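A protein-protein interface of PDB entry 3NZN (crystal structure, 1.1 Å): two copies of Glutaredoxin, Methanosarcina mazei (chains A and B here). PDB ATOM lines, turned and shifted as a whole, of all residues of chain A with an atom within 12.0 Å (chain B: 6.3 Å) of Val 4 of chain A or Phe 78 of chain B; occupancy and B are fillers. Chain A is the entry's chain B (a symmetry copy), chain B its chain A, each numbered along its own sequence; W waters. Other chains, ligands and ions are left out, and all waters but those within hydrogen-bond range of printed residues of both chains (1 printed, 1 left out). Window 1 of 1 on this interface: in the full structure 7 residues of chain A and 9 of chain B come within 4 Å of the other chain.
The side-chain hydroxyl (OG) of Ser 75 of chain B sits at hydrogen-bond distance from the side-chain amide nitrogen (ND2) of Asn 14 of chain A (3.1 Å). N of Phe 78 of chain B is in hydrogen-bond range of O of Val 4 of chain A, at 2.8 Å.
The side-chain sulfur (SG) of Cys 35 of chain B lies within hydrogen-bond range of the backbone NH (N) of Leu 29 of chain B, 3.6 Å away. O of Ser 77 of chain B lies within hydrogen-bond range of OG1 of Thr 80 of chain B (2.7 Å). The side-chain hydroxyl (OG) of Ser 1 of chain A is in hydrogen-bond range of the backbone NH (N) of Ala 3 of chain A, 3.0 Å away. N of Ser 1 of chain A sits at hydrogen-bond distance from OD2 of Asp 11 of chain A, 2.8 Å away. The side-chain amide oxygen (OD1) of Asn 5 of chain A is in hydrogen-bond range of the backbone NH (N) of Gly 8 of chain A (3.0 Å). The side-chain sulfur (SG) of Cys 32 of chain B forms a disulfide with the side-chain sulfur (SG) of Cys 35 of chain B (2.3 Å).
Water W1 bridges the backbone carbonyl oxygen of Val 76 of chain B (2.7 Å) and the backbone NH of Leu 6 of chain A (2.9 Å).
Gly 91 of chain B touches Ser 1 of chain A. Trp 34 of chain B touches Asn 2 of chain A (CD1 to O, 3.5 Å). Ser 77 of chain B touches Ala 3 of chain A. CA of Ala 3 of chain A touches O of Phe 78 of chain B, at 3.1 Å. Val 4 of chain A touches Ser 77 of chain B. Asn 5 of chain A touches Leu 29 of chain B. Asn 5 of chain A touches Phe 78 of chain B. Leu 29 of chain B touches Leu 6 of chain A. N of Leu 6 of chain A touches O of Val 76 of chain B, at 3.7 Å. Leu 6 of chain A touches Phe 78 of chain B (CD2 to CE2, 3.6 Å).
No position is printed for both chains. Of the 17 pairs that touch across the chains among the printed residues, none has its exchanged pair printed and touching as well.
Of the 20 printed residues of chain B, 8 touch a printed residue of chain A. Printed residues of chain B that touch a printed residue of chain A: Leu 29, Trp 34, Ser 75, Val 76, Ser 77, Phe 78, Val 90 and Gly 91. Hydrophobic or aromatic side chains of chain B within 4 Å of the printed part of chain A: Leu 29, Trp 34, Phe 78 and Val 90. Of the 17 printed residues of chain A, 7 touch a printed residue of chain B. Hydrophobic or aromatic side chains of chain A that line the printed part of chain B: Ala 3, Val 4 and Leu 6. Along chain A the printed residues that touch a printed residue of chain B span positions 1 to 14. Among the printed residues, 17 pairs touch across the chains. Among the printed residues, no Asp or Glu carboxylate lies within 4 Å of a Lys or Arg side-chain nitrogen of the other chain.
Printed residues of chain B within 4 Å of Ser 1 of chain A: Val 90 and Gly 91. Of the printed residues of chain B, Ala 3 of chain A touches Ser 77, Phe 78 and Val 90. Printed residues of chain B within 4 Å of Val 4 of chain A: Leu 29 (3.9 Å), Ser 77 (3.1 Å) and Phe 78 (2.8 Å). Printed residues of chain B within 4 Å of Leu 6 of chain A: Leu 29, Val 76 and Phe 78. No residue of chain A comes within 4 Å of Gly 28 of chain B. No residue of chain A comes within 4 Å of Cys 32 of chain B. No residue of chain A comes within 4 Å of Cys 35 of chain B. No residue of chain A comes within 4 Å of Val 54 of chain B. No residue of chain A comes within 4 Å of Val 69 of chain B. Of the printed residues of chain A, Ser 75 of chain B touches Asn 14 (3.1 Å). Phe 78 of chain B touches just these residues of chain A: Ala 3, Val 4, Asn 5 and Leu 6. No residue of chain A comes within 4 Å of Pro 79 of chain B. Of chain A, only Ser 1 and Ala 3 come within 4 Å of Val 90 of chain B. Of chain A, only Ser 1 (3.9 Å) and Asn 2 (3.4 Å) come within 4 Å of Gly 91 of chain B. The nearest residue of chain B that does not touch Val 4 of chain A is Cys 32 of chain B (4.2 Å). The nearest residue of chain A that does not touch Phe 78 of chain B is Asn 2 of chain A (4.5 Å).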
ATOM      1  N   SER A   1      24.210 -18.888  11.543  1.00  0.00           N
ATOM      2  CA  SER A   1      25.565 -19.500  11.762  1.00  0.00           C
ATOM      3  C   SER A   1      25.303 -20.928  12.178  1.00  0.00           C
ATOM      4  O   SER A   1      24.216 -21.180  12.596  1.00  0.00           O
ATOM      5  CB  SER A   1      26.116 -18.772  13.010  1.00  0.00           C
ATOM      6  OG  SER A   1      27.281 -19.375  13.482  1.00  0.00           O
ATOM      7  N   ASN A   2      26.281 -21.828  12.224  1.00  0.00           N
ATOM      8  CA  ASN A   2      26.127 -23.133  12.898  1.00  0.00           C
ATOM      9  C   ASN A   2      26.383 -23.078  14.406  1.00  0.00           C
ATOM     10  O   ASN A   2      26.299 -24.084  15.099  1.00  0.00           O
ATOM     11  CB  ASN A   2      26.905 -24.197  12.213  1.00  0.00           C
ATOM     12  CG  ASN A   2      28.404 -23.831  12.023  1.00  0.00           C
ATOM     13  OD1 ASN A   2      29.007 -24.060  10.991  1.00  0.00           O
ATOM     14  ND2 ASN A   2      29.000 -23.410  13.086  1.00  0.00           N
ATOM     15  N   ALA A   3      26.588 -21.878  14.952  1.00  0.00           N
ATOM     16  CA  ALA A   3      26.817 -21.746  16.371  1.00  0.00           C
ATOM     17  C   ALA A   3      25.491 -22.070  17.112  1.00  0.00           C
ATOM     18  O   ALA A   3      24.384 -21.841  16.606  1.00  0.00           O
ATOM     19  CB  ALA A   3      27.296 -20.333  16.669  1.00  0.00           C
ATOM     20  N   VAL A   4      25.617 -22.552  18.344  1.00  0.00           N
ATOM     21  CA  VAL A   4      24.494 -22.785  19.261  1.00  0.00           C
ATOM     22  C   VAL A   4      24.582 -21.902  20.461  1.00  0.00           C
ATOM     23  O   VAL A   4      25.660 -21.416  20.820  1.00  0.00           O
ATOM     24  CB  VAL A   4      24.450 -24.268  19.671  1.00  0.00           C
ATOM     25  CG1 VAL A   4      24.241 -25.230  18.482  1.00  0.00           C
ATOM     26  CG2 VAL A   4      25.600 -24.686  20.571  1.00  0.00           C
ATOM     27  N   ASN A   5      23.442 -21.671  21.152  1.00  0.00           N
ATOM     28  CA  ASN A   5      23.442 -20.867  22.319  1.00  0.00           C
ATOM     29  C   ASN A   5      23.927 -21.637  23.502  1.00  0.00           C
ATOM     30  O   ASN A   5      24.278 -22.800  23.397  1.00  0.00           O
ATOM     31  CB  ASN A   5      22.097 -20.150  22.491  1.00  0.00           C
ATOM     32  CG  ASN A   5      20.972 -21.036  22.922  1.00  0.00           C
ATOM     33  OD1 ASN A   5      21.191 -22.187  23.271  1.00  0.00           O
ATOM     34  ND2 ASN A   5      19.794 -20.438  23.069  1.00  0.00           N
ATOM     35  N   LEU A   6      23.940 -20.985  24.670  1.00  0.00           N
ATOM     36  CA  LEU A   6      24.394 -21.619  25.874  1.00  0.00           C
ATOM     37  C   LEU A   6      23.669 -22.919  26.208  1.00  0.00           C
ATOM     38  O   LEU A   6      24.212 -23.805  26.885  1.00  0.00           O
ATOM     39  CB  LEU A   6      24.245 -20.742  27.076  1.00  0.00           C
ATOM     40  CG  LEU A   6      25.233 -20.060  27.781  1.00  0.00           C
ATOM     41  CD1 LEU A   6      24.740 -19.428  28.950  1.00  0.00           C
ATOM     42  CD2 LEU A   6      26.542 -20.757  28.072  1.00  0.00           C
ATOM     43  N   PHE A   7      22.413 -22.942  25.785  1.00  0.00           N
ATOM     44  CA  PHE A   7      21.520 -23.989  26.076  1.00  0.00           C
ATOM     45  C   PHE A   7      21.414 -25.003  24.967  1.00  0.00           C
ATOM     46  O   PHE A   7      20.561 -25.903  25.001  1.00  0.00           O
ATOM     47  CB  PHE A   7      20.097 -23.410  26.423  1.00  0.00           C
ATOM     48  CG  PHE A   7      20.166 -22.305  27.444  1.00  0.00           C
ATOM     49  CD1 PHE A   7      20.348 -22.668  28.802  1.00  0.00           C
ATOM     50  CD2 PHE A   7      20.169 -21.033  27.075  1.00  0.00           C
ATOM     51  CE1 PHE A   7      20.537 -21.718  29.718  1.00  0.00           C
ATOM     52  CE2 PHE A   7      20.361 -20.074  28.016  1.00  0.00           C
ATOM     53  CZ  PHE A   7      20.524 -20.431  29.339  1.00  0.00           C
ATOM     54  N   GLY A   8      22.340 -24.906  23.996  1.00  0.00           N
ATOM     55  CA  GLY A   8      22.451 -25.856  22.941  1.00  0.00           C
ATOM     56  C   GLY A   8      21.527 -25.675  21.758  1.00  0.00           C
ATOM     57  O   GLY A   8      21.530 -26.523  20.853  1.00  0.00           O
ATOM     58  N   GLN A   9      20.746 -24.626  21.733  1.00  0.00           N
ATOM     59  CA  GLN A   9      19.825 -24.387  20.642  1.00  0.00           C
ATOM     60  C   GLN A   9      20.530 -23.794  19.416  1.00  0.00           C
ATOM     61  O   GLN A   9      21.359 -22.926  19.536  1.00  0.00           O
ATOM     62  CB  GLN A   9      18.719 -23.452  21.130  1.00  0.00           C
ATOM     63  CG  GLN A   9      17.812 -24.020  22.185  1.00  0.00           C
ATOM     64  CD  GLN A   9      16.491 -24.701  21.628  1.00  0.00           C
ATOM     65  OE1 GLN A   9      16.214 -24.697  20.415  1.00  0.00           O
ATOM     66  NE2 GLN A   9      15.679 -25.253  22.527  1.00  0.00           N
ATOM     67  N   LYS A  10      20.181 -24.281  18.241  1.00  0.00           N
ATOM     68  CA  LYS A  10      20.616 -23.691  17.004  1.00  0.00           C
ATOM     69  C   LYS A  10      20.171 -22.306  16.786  1.00  0.00           C
ATOM     70  O   LYS A  10      19.258 -21.848  17.449  1.00  0.00           O
ATOM     71  CB  LYS A  10      20.161 -24.509  15.815  1.00  0.00           C
ATOM     72  CG  LYS A  10      20.616 -25.956  15.798  1.00  0.00           C
ATOM     73  CD  LYS A  10      20.322 -26.719  14.442  1.00  0.00           C
ATOM     74  CE  LYS A  10      18.845 -27.280  14.386  1.00  0.00           C
ATOM     75  NZ  LYS A  10      18.517 -28.399  15.371  1.00  0.00           N
ATOM     76  N   ASP A  11      20.869 -21.596  15.943  1.00  0.00           N
ATOM     77  CA  ASP A  11      20.683 -20.206  15.599  1.00  0.00           C
ATOM     78  C   ASP A  11      19.351 -20.067  14.884  1.00  0.00           C
ATOM     79  O   ASP A  11      19.199 -20.438  13.745  1.00  0.00           O
ATOM     80  CB  ASP A  11      21.850 -19.687  14.709  1.00  0.00           C
ATOM     81  CG  ASP A  11      21.739 -18.217  14.410  1.00  0.00           C
ATOM     82  OD1 ASP A  11      20.872 -17.519  14.910  1.00  0.00           O
ATOM     83  OD2 ASP A  11      22.613 -17.836  13.607  1.00  0.00           O
ATOM     84  N   ARG A  12      18.390 -19.469  15.565  1.00  0.00           N
ATOM     85  CA  ARG A  12      17.061 -19.301  15.061  1.00  0.00           C
ATOM     86  C   ARG A  12      16.822 -17.875  14.627  1.00  0.00           C
ATOM     87  O   ARG A  12      15.780 -17.524  14.169  1.00  0.00           O
ATOM     88  CB  ARG A  12      16.016 -19.724  16.065  1.00  0.00           C
ATOM     89  CG  ARG A  12      16.019 -21.239  16.321  1.00  0.00           C
ATOM     90  CD  ARG A  12      15.539 -21.630  17.647  1.00  0.00           C
ATOM     91  NE  ARG A  12      16.465 -21.099  18.636  1.00  0.00           N
ATOM     92  CZ  ARG A  12      16.143 -20.798  19.842  1.00  0.00           C
ATOM     93  NH1 ARG A  12      16.995 -20.168  20.635  1.00  0.00           N
ATOM     94  NH2 ARG A  12      14.931 -21.059  20.331  1.00  0.00           N
ATOM     95  N   GLY A  13      17.833 -16.997  14.809  1.00  0.00           N
ATOM     96  CA  GLY A  13      17.735 -15.570  14.571  1.00  0.00           C
ATOM     97  C   GLY A  13      18.231 -14.777  15.737  1.00  0.00           C
ATOM     98  O   GLY A  13      18.863 -15.292  16.622  1.00  0.00           O
ATOM     99  N   ASN A  14      17.964 -13.493  15.701  1.00  0.00           N
ATOM    100  CA  ASN A  14      18.515 -12.610  16.697  1.00  0.00           C
ATOM    101  C   ASN A  14      17.863 -11.246  16.648  1.00  0.00           C
ATOM    102  O   ASN A  14      17.064 -10.925  15.752  1.00  0.00           O
ATOM    103  CB  ASN A  14      20.055 -12.488  16.604  1.00  0.00           C
ATOM    104  CG  ASN A  14      20.654 -12.627  17.947  1.00  0.00           C
ATOM    105  OD1 ASN A  14      20.271 -11.929  18.894  1.00  0.00           O
ATOM    106  ND2 ASN A  14      21.584 -13.520  18.075  1.00  0.00           N
ATOM    107  N   TYR A  51      15.539 -10.700  13.321  1.00  0.00           N
ATOM    108  CA  TYR A  51      15.441 -11.635  12.233  1.00  0.00           C
ATOM    109  C   TYR A  51      15.221 -13.032  12.790  1.00  0.00           C
ATOM    110  O   TYR A  51      15.770 -13.382  13.804  1.00  0.00           O
ATOM    111  CB  TYR A  51      16.596 -11.541  11.251  1.00  0.00           C
ATOM    112  CG  TYR A  51      17.893 -11.838  11.855  1.00  0.00           C
ATOM    113  CD1 TYR A  51      18.426 -13.063  11.781  1.00  0.00           C
ATOM    114  CD2 TYR A  51      18.593 -10.878  12.587  1.00  0.00           C
ATOM    115  CE1 TYR A  51      19.705 -13.400  12.245  1.00  0.00           C
ATOM    116  CE2 TYR A  51      19.863 -11.167  13.159  1.00  0.00           C
ATOM    117  CZ  TYR A  51      20.426 -12.441  12.992  1.00  0.00           C
ATOM    118  OH  TYR A  51      21.600 -12.819  13.543  1.00  0.00           O
ATOM    119  N   TYR A  53      14.786 -17.177  11.531  1.00  0.00           N
ATOM    120  CA  TYR A  53      14.889 -18.221  10.547  1.00  0.00           C
ATOM    121  C   TYR A  53      13.783 -19.270  10.753  1.00  0.00           C
ATOM    122  O   TYR A  53      13.842 -20.087  11.649  1.00  0.00           O
ATOM    123  CB  TYR A  53      16.239 -18.869  10.638  1.00  0.00           C
ATOM    124  CG  TYR A  53      17.404 -17.954  10.383  1.00  0.00           C
ATOM    125  CD1 TYR A  53      17.390 -17.012   9.353  1.00  0.00           C
ATOM    126  CD2 TYR A  53      18.498 -17.977  11.182  1.00  0.00           C
ATOM    127  CE1 TYR A  53      18.505 -16.206   9.100  1.00  0.00           C
ATOM    128  CE2 TYR A  53      19.578 -17.172  10.985  1.00  0.00           C
ATOM    129  CZ  TYR A  53      19.565 -16.259   9.920  1.00  0.00           C
ATOM    130  OH  TYR A  53      20.662 -15.414   9.681  1.00  0.00           O
ATOM    131  N   ARG A  56      14.136 -22.929  11.279  1.00  0.00           N
ATOM    132  CA  ARG A  56      14.804 -23.416  12.506  1.00  0.00           C
ATOM    133  C   ARG A  56      13.859 -23.409  13.698  1.00  0.00           C
ATOM    134  O   ARG A  56      14.230 -23.813  14.801  1.00  0.00           O
ATOM    135  CB  ARG A  56      15.991 -22.546  12.795  1.00  0.00           C
ATOM    136  CG  ARG A  56      17.077 -22.667  11.712  1.00  0.00           C
ATOM    137  CD  ARG A  56      18.377 -23.191  12.246  1.00  0.00           C
ATOM    138  NE  ARG A  56      19.420 -23.564  11.302  1.00  0.00           N
ATOM    139  CZ  ARG A  56      20.509 -22.864  11.075  1.00  0.00           C
ATOM    140  NH1 ARG A  56      21.340 -23.368  10.170  1.00  0.00           N
ATOM    141  NH2 ARG A  56      20.769 -21.697  11.679  1.00  0.00           N
ATOM    142  N   TYR B  27      36.115 -21.053  22.918  1.00  0.00           N
ATOM    143  CA  TYR B  27      35.025 -21.309  23.883  1.00  0.00           C
ATOM    144  C   TYR B  27      33.955 -22.166  23.211  1.00  0.00           C
ATOM    145  O   TYR B  27      33.454 -21.845  22.234  1.00  0.00           O
ATOM    146  CB  TYR B  27      34.441 -20.010  24.402  1.00  0.00           C
ATOM    147  CG  TYR B  27      35.447 -19.257  25.232  1.00  0.00           C
ATOM    148  CD1 TYR B  27      35.560 -19.482  26.597  1.00  0.00           C
ATOM    149  CD2 TYR B  27      36.258 -18.285  24.673  1.00  0.00           C
ATOM    150  CE1 TYR B  27      36.487 -18.780  27.366  1.00  0.00           C
ATOM    151  CE2 TYR B  27      37.190 -17.592  25.454  1.00  0.00           C
ATOM    152  CZ  TYR B  27      37.289 -17.844  26.756  1.00  0.00           C
ATOM    153  OH  TYR B  27      38.233 -17.081  27.414  1.00  0.00           O
ATOM    154  N   GLY B  28      33.668 -23.290  23.880  1.00  0.00           N
ATOM    155  CA  GLY B  28      32.689 -24.202  23.341  1.00  0.00           C
ATOM    156  C   GLY B  28      31.801 -24.826  24.430  1.00  0.00           C
ATOM    157  O   GLY B  28      31.893 -24.432  25.600  1.00  0.00           O
ATOM    158  N   LEU B  29      31.017 -25.790  24.042  1.00  0.00           N
ATOM    159  CA  LEU B  29      30.244 -26.618  24.964  1.00  0.00           C
ATOM    160  C   LEU B  29      30.686 -28.067  24.761  1.00  0.00           C
ATOM    161  O   LEU B  29      31.016 -28.451  23.642  1.00  0.00           O
ATOM    162  CB  LEU B  29      28.739 -26.501  24.662  1.00  0.00           C
ATOM    163  CG  LEU B  29      28.134 -25.111  24.701  1.00  0.00           C
ATOM    164  CD1 LEU B  29      26.681 -25.063  24.302  1.00  0.00           C
ATOM    165  CD2 LEU B  29      28.361 -24.363  26.010  1.00  0.00           C
ATOM    166  N   THR B  31      28.957 -30.702  24.629  1.00  0.00           N
ATOM    167  CA  THR B  31      27.947 -31.269  23.728  1.00  0.00           C
ATOM    168  C   THR B  31      27.731 -30.276  22.618  1.00  0.00           C
ATOM    169  O   THR B  31      27.037 -29.324  22.830  1.00  0.00           O
ATOM    170  CB  THR B  31      26.620 -31.334  24.458  1.00  0.00           C
ATOM    171  OG1 THR B  31      26.383 -29.930  24.760  1.00  0.00           O
ATOM    172  CG2 THR B  31      26.770 -32.189  25.630  1.00  0.00           C
ATOM    173  N   CYS B  32      28.533 -30.213  21.606  1.00  0.00           N
ATOM    174  CA  CYS B  32      28.386 -29.238  20.539  1.00  0.00           C
ATOM    175  C   CYS B  32      29.241 -29.796  19.377  1.00  0.00           C
ATOM    176  O   CYS B  32      30.456 -29.750  19.375  1.00  0.00           O
ATOM    177  CB  CYS B  32      28.889 -27.872  20.953  1.00  0.00           C
ATOM    178  SG  CYS B  32      29.194 -26.615  19.754  1.00  0.00           S
ATOM    179  N   TRP B  34      29.668 -28.745  16.328  1.00  0.00           N
ATOM    180  CA  TRP B  34      30.468 -27.789  15.630  1.00  0.00           C
ATOM    181  C   TRP B  34      31.671 -27.313  16.403  1.00  0.00           C
ATOM    182  O   TRP B  34      32.685 -26.927  15.822  1.00  0.00           O
ATOM    183  CB  TRP B  34      29.636 -26.686  15.064  1.00  0.00           C
ATOM    184  CG  TRP B  34      28.628 -27.149  14.067  1.00  0.00           C
ATOM    185  CD1 TRP B  34      27.301 -27.305  14.263  1.00  0.00           C
ATOM    186  CD2 TRP B  34      28.904 -27.434  12.692  1.00  0.00           C
ATOM    187  NE1 TRP B  34      26.707 -27.691  13.089  1.00  0.00           N
ATOM    188  CE2 TRP B  34      27.677 -27.807  12.129  1.00  0.00           C
ATOM    189  CE3 TRP B  34      30.070 -27.500  11.909  1.00  0.00           C
ATOM    190  CZ2 TRP B  34      27.568 -28.152  10.805  1.00  0.00           C
ATOM    191  CZ3 TRP B  34      29.930 -27.804  10.572  1.00  0.00           C
ATOM    192  CH2 TRP B  34      28.706 -28.121  10.040  1.00  0.00           C
ATOM    193  N   CYS B  35      31.548 -27.329  17.731  1.00  0.00           N
ATOM    194  CA  CYS B  35      32.683 -27.052  18.589  1.00  0.00           C
ATOM    195  C   CYS B  35      33.701 -28.137  18.394  1.00  0.00           C
ATOM    196  O   CYS B  35      34.915 -27.870  18.260  1.00  0.00           O
ATOM    197  CB  CYS B  35      32.303 -26.953  20.028  1.00  0.00           C
ATOM    198  SG  CYS B  35      31.151 -25.661  20.473  1.00  0.00           S
ATOM    199  N   VAL B  52      37.918 -24.299  26.048  1.00  0.00           N
ATOM    200  CA  VAL B  52      37.134 -24.269  27.340  1.00  0.00           C
ATOM    201  C   VAL B  52      35.751 -24.738  26.989  1.00  0.00           C
ATOM    202  O   VAL B  52      35.115 -24.297  26.071  1.00  0.00           O
ATOM    203  CB  VAL B  52      37.069 -22.816  27.836  1.00  0.00           C
ATOM    204  CG1 VAL B  52      36.198 -22.708  29.115  1.00  0.00           C
ATOM    205  CG2 VAL B  52      38.498 -22.292  28.126  1.00  0.00           C
ATOM    206  N   VAL B  54      32.395 -24.377  28.434  1.00  0.00           N
ATOM    207  CA  VAL B  54      31.785 -23.418  29.347  1.00  0.00           C
ATOM    208  C   VAL B  54      30.652 -24.185  30.204  1.00  0.00           C
ATOM    209  O   VAL B  54      30.542 -23.799  31.411  1.00  0.00           O
ATOM    210  CB  VAL B  54      31.167 -22.257  28.615  1.00  0.00           C
ATOM    211  CG1 VAL B  54      30.405 -21.338  29.498  1.00  0.00           C
ATOM    212  CG2 VAL B  54      32.286 -21.388  27.907  1.00  0.00           C
ATOM    213  N   VAL B  66      31.662 -16.700  30.397  1.00  0.00           N
ATOM    214  CA  VAL B  66      30.573 -16.131  29.671  1.00  0.00           C
ATOM    215  C   VAL B  66      30.823 -14.670  29.393  1.00  0.00           C
ATOM    216  O   VAL B  66      30.500 -14.182  28.316  1.00  0.00           O
ATOM    217  CB  VAL B  66      29.226 -16.387  30.381  1.00  0.00           C
ATOM    218  CG1 VAL B  66      28.166 -15.506  29.763  1.00  0.00           C
ATOM    219  CG2 VAL B  66      28.929 -17.917  30.343  1.00  0.00           C
ATOM    220  N   VAL B  69      33.202 -14.454  26.409  1.00  0.00           N
ATOM    221  CA  VAL B  69      32.502 -14.716  25.188  1.00  0.00           C
ATOM    222  C   VAL B  69      31.625 -13.530  24.818  1.00  0.00           C
ATOM    223  O   VAL B  69      31.606 -13.068  23.718  1.00  0.00           O
ATOM    224  CB  VAL B  69      31.674 -16.001  25.292  1.00  0.00           C
ATOM    225  CG1 VAL B  69      30.821 -16.177  24.081  1.00  0.00           C
ATOM    226  CG2 VAL B  69      32.588 -17.180  25.463  1.00  0.00           C
ATOM    227  N   ASN B  73      31.356 -11.613  21.373  1.00  0.00           N
ATOM    228  CA  ASN B  73      30.230 -12.259  20.705  1.00  0.00           C
ATOM    229  C   ASN B  73      28.988 -12.063  21.593  1.00  0.00           C
ATOM    230  O   ASN B  73      28.648 -12.879  22.412  1.00  0.00           O
ATOM    231  CB  ASN B  73      30.456 -13.742  20.523  1.00  0.00           C
ATOM    232  CG  ASN B  73      29.226 -14.445  19.975  1.00  0.00           C
ATOM    233  OD1 ASN B  73      28.329 -13.810  19.471  1.00  0.00           O
ATOM    234  ND2 ASN B  73      29.252 -15.748  19.981  1.00  0.00           N
ATOM    235  N   SER B  75      25.980 -12.528  21.180  1.00  0.00           N
ATOM    236  CA  SER B  75      25.024 -13.623  21.110  1.00  0.00           C
ATOM    237  C   SER B  75      25.273 -14.690  22.180  1.00  0.00           C
ATOM    238  O   SER B  75      24.402 -15.590  22.410  1.00  0.00           O
ATOM    239  CB  SER B  75      24.925 -14.239  19.743  1.00  0.00           C
ATOM    240  OG  SER B  75      24.550 -13.321  18.809  1.00  0.00           O
ATOM    241  N   VAL B  76      26.489 -14.757  22.716  1.00  0.00           N
ATOM    242  CA  VAL B  76      26.885 -15.838  23.611  1.00  0.00           C
ATOM    243  C   VAL B  76      26.506 -17.158  23.013  1.00  0.00           C
ATOM    244  O   VAL B  76      25.732 -17.979  23.506  1.00  0.00           O
ATOM    245  CB  VAL B  76      26.354 -15.623  25.039  1.00  0.00           C
ATOM    246  CG1 VAL B  76      26.999 -16.577  25.972  1.00  0.00           C
ATOM    247  CG2 VAL B  76      26.599 -14.164  25.431  1.00  0.00           C
ATOM    248  N   SER B  77      27.219 -17.445  21.900  1.00  0.00           N
ATOM    249  CA  SER B  77      27.028 -18.642  21.124  1.00  0.00           C
ATOM    250  C   SER B  77      28.377 -19.349  20.923  1.00  0.00           C
ATOM    251  O   SER B  77      29.433 -18.767  21.140  1.00  0.00           O
ATOM    252  CB  SER B  77      26.319 -18.369  19.861  1.00  0.00           C
ATOM    253  OG  SER B  77      27.089 -17.520  19.012  1.00  0.00           O
ATOM    254  N   PHE B  78      28.280 -20.588  20.496  1.00  0.00           N
ATOM    255  CA  PHE B  78      29.422 -21.510  20.559  1.00  0.00           C
ATOM    256  C   PHE B  78      29.500 -22.335  19.279  1.00  0.00           C
ATOM    257  O   PHE B  78      28.488 -22.832  18.789  1.00  0.00           O
ATOM    258  CB  PHE B  78      29.252 -22.472  21.750  1.00  0.00           C
ATOM    259  CG  PHE B  78      29.162 -21.703  23.024  1.00  0.00           C
ATOM    260  CD1 PHE B  78      30.300 -21.248  23.673  1.00  0.00           C
ATOM    261  CD2 PHE B  78      27.927 -21.287  23.583  1.00  0.00           C
ATOM    262  CE1 PHE B  78      30.229 -20.481  24.780  1.00  0.00           C
ATOM    263  CE2 PHE B  78      27.888 -20.499  24.708  1.00  0.00           C
ATOM    264  CZ  PHE B  78      28.985 -20.093  25.277  1.00  0.00           C
ATOM    265  N   PRO B  79      30.715 -22.541  18.716  1.00  0.00           N
ATOM    266  CA  PRO B  79      31.932 -22.057  19.275  1.00  0.00           C
ATOM    267  C   PRO B  79      32.184 -20.574  19.037  1.00  0.00           C
ATOM    268  O   PRO B  79      31.718 -20.017  18.061  1.00  0.00           O
ATOM    269  CB  PRO B  79      32.996 -22.845  18.469  1.00  0.00           C
ATOM    270  CG  PRO B  79      32.314 -23.174  17.167  1.00  0.00           C
ATOM    271  CD  PRO B  79      30.856 -23.406  17.578  1.00  0.00           C
ATOM    272  N   THR B  80      32.939 -19.952  19.935  1.00  0.00           N
ATOM    273  CA  THR B  80      33.539 -18.634  19.702  1.00  0.00           C
ATOM    274  C   THR B  80      35.053 -18.849  19.895  1.00  0.00           C
ATOM    275  O   THR B  80      35.544 -19.222  20.930  1.00  0.00           O
ATOM    276  CB  THR B  80      33.042 -17.593  20.660  1.00  0.00           C
ATOM    277  OG1 THR B  80      31.638 -17.383  20.470  1.00  0.00           O
ATOM    278  CG2 THR B  80      33.674 -16.312  20.484  1.00  0.00           C
ATOM    279  N   VAL B  90      32.768 -16.727  15.077  1.00  0.00           N
ATOM    280  CA  VAL B  90      31.581 -17.365  15.680  1.00  0.00           C
ATOM    281  C   VAL B  90      31.161 -18.463  14.750  1.00  0.00           C
ATOM    282  O   VAL B  90      30.862 -18.217  13.599  1.00  0.00           O
ATOM    283  CB  VAL B  90      30.555 -16.335  15.923  1.00  0.00           C
ATOM    284  CG1 VAL B  90      29.268 -17.029  16.510  1.00  0.00           C
ATOM    285  CG2 VAL B  90      31.025 -15.270  16.922  1.00  0.00           C
ATOM    286  N   GLY B  91      31.053 -19.696  15.269  1.00  0.00           N
ATOM    287  CA  GLY B  91      30.737 -20.855  14.496  1.00  0.00           C
ATOM    288  C   GLY B  91      31.964 -21.538  13.902  1.00  0.00           C
ATOM    289  O   GLY B  91      33.053 -21.024  13.934  1.00  0.00           O
HETATM  290  O   HOH W   1      23.412 -18.171  24.828  1.00  0.00           O
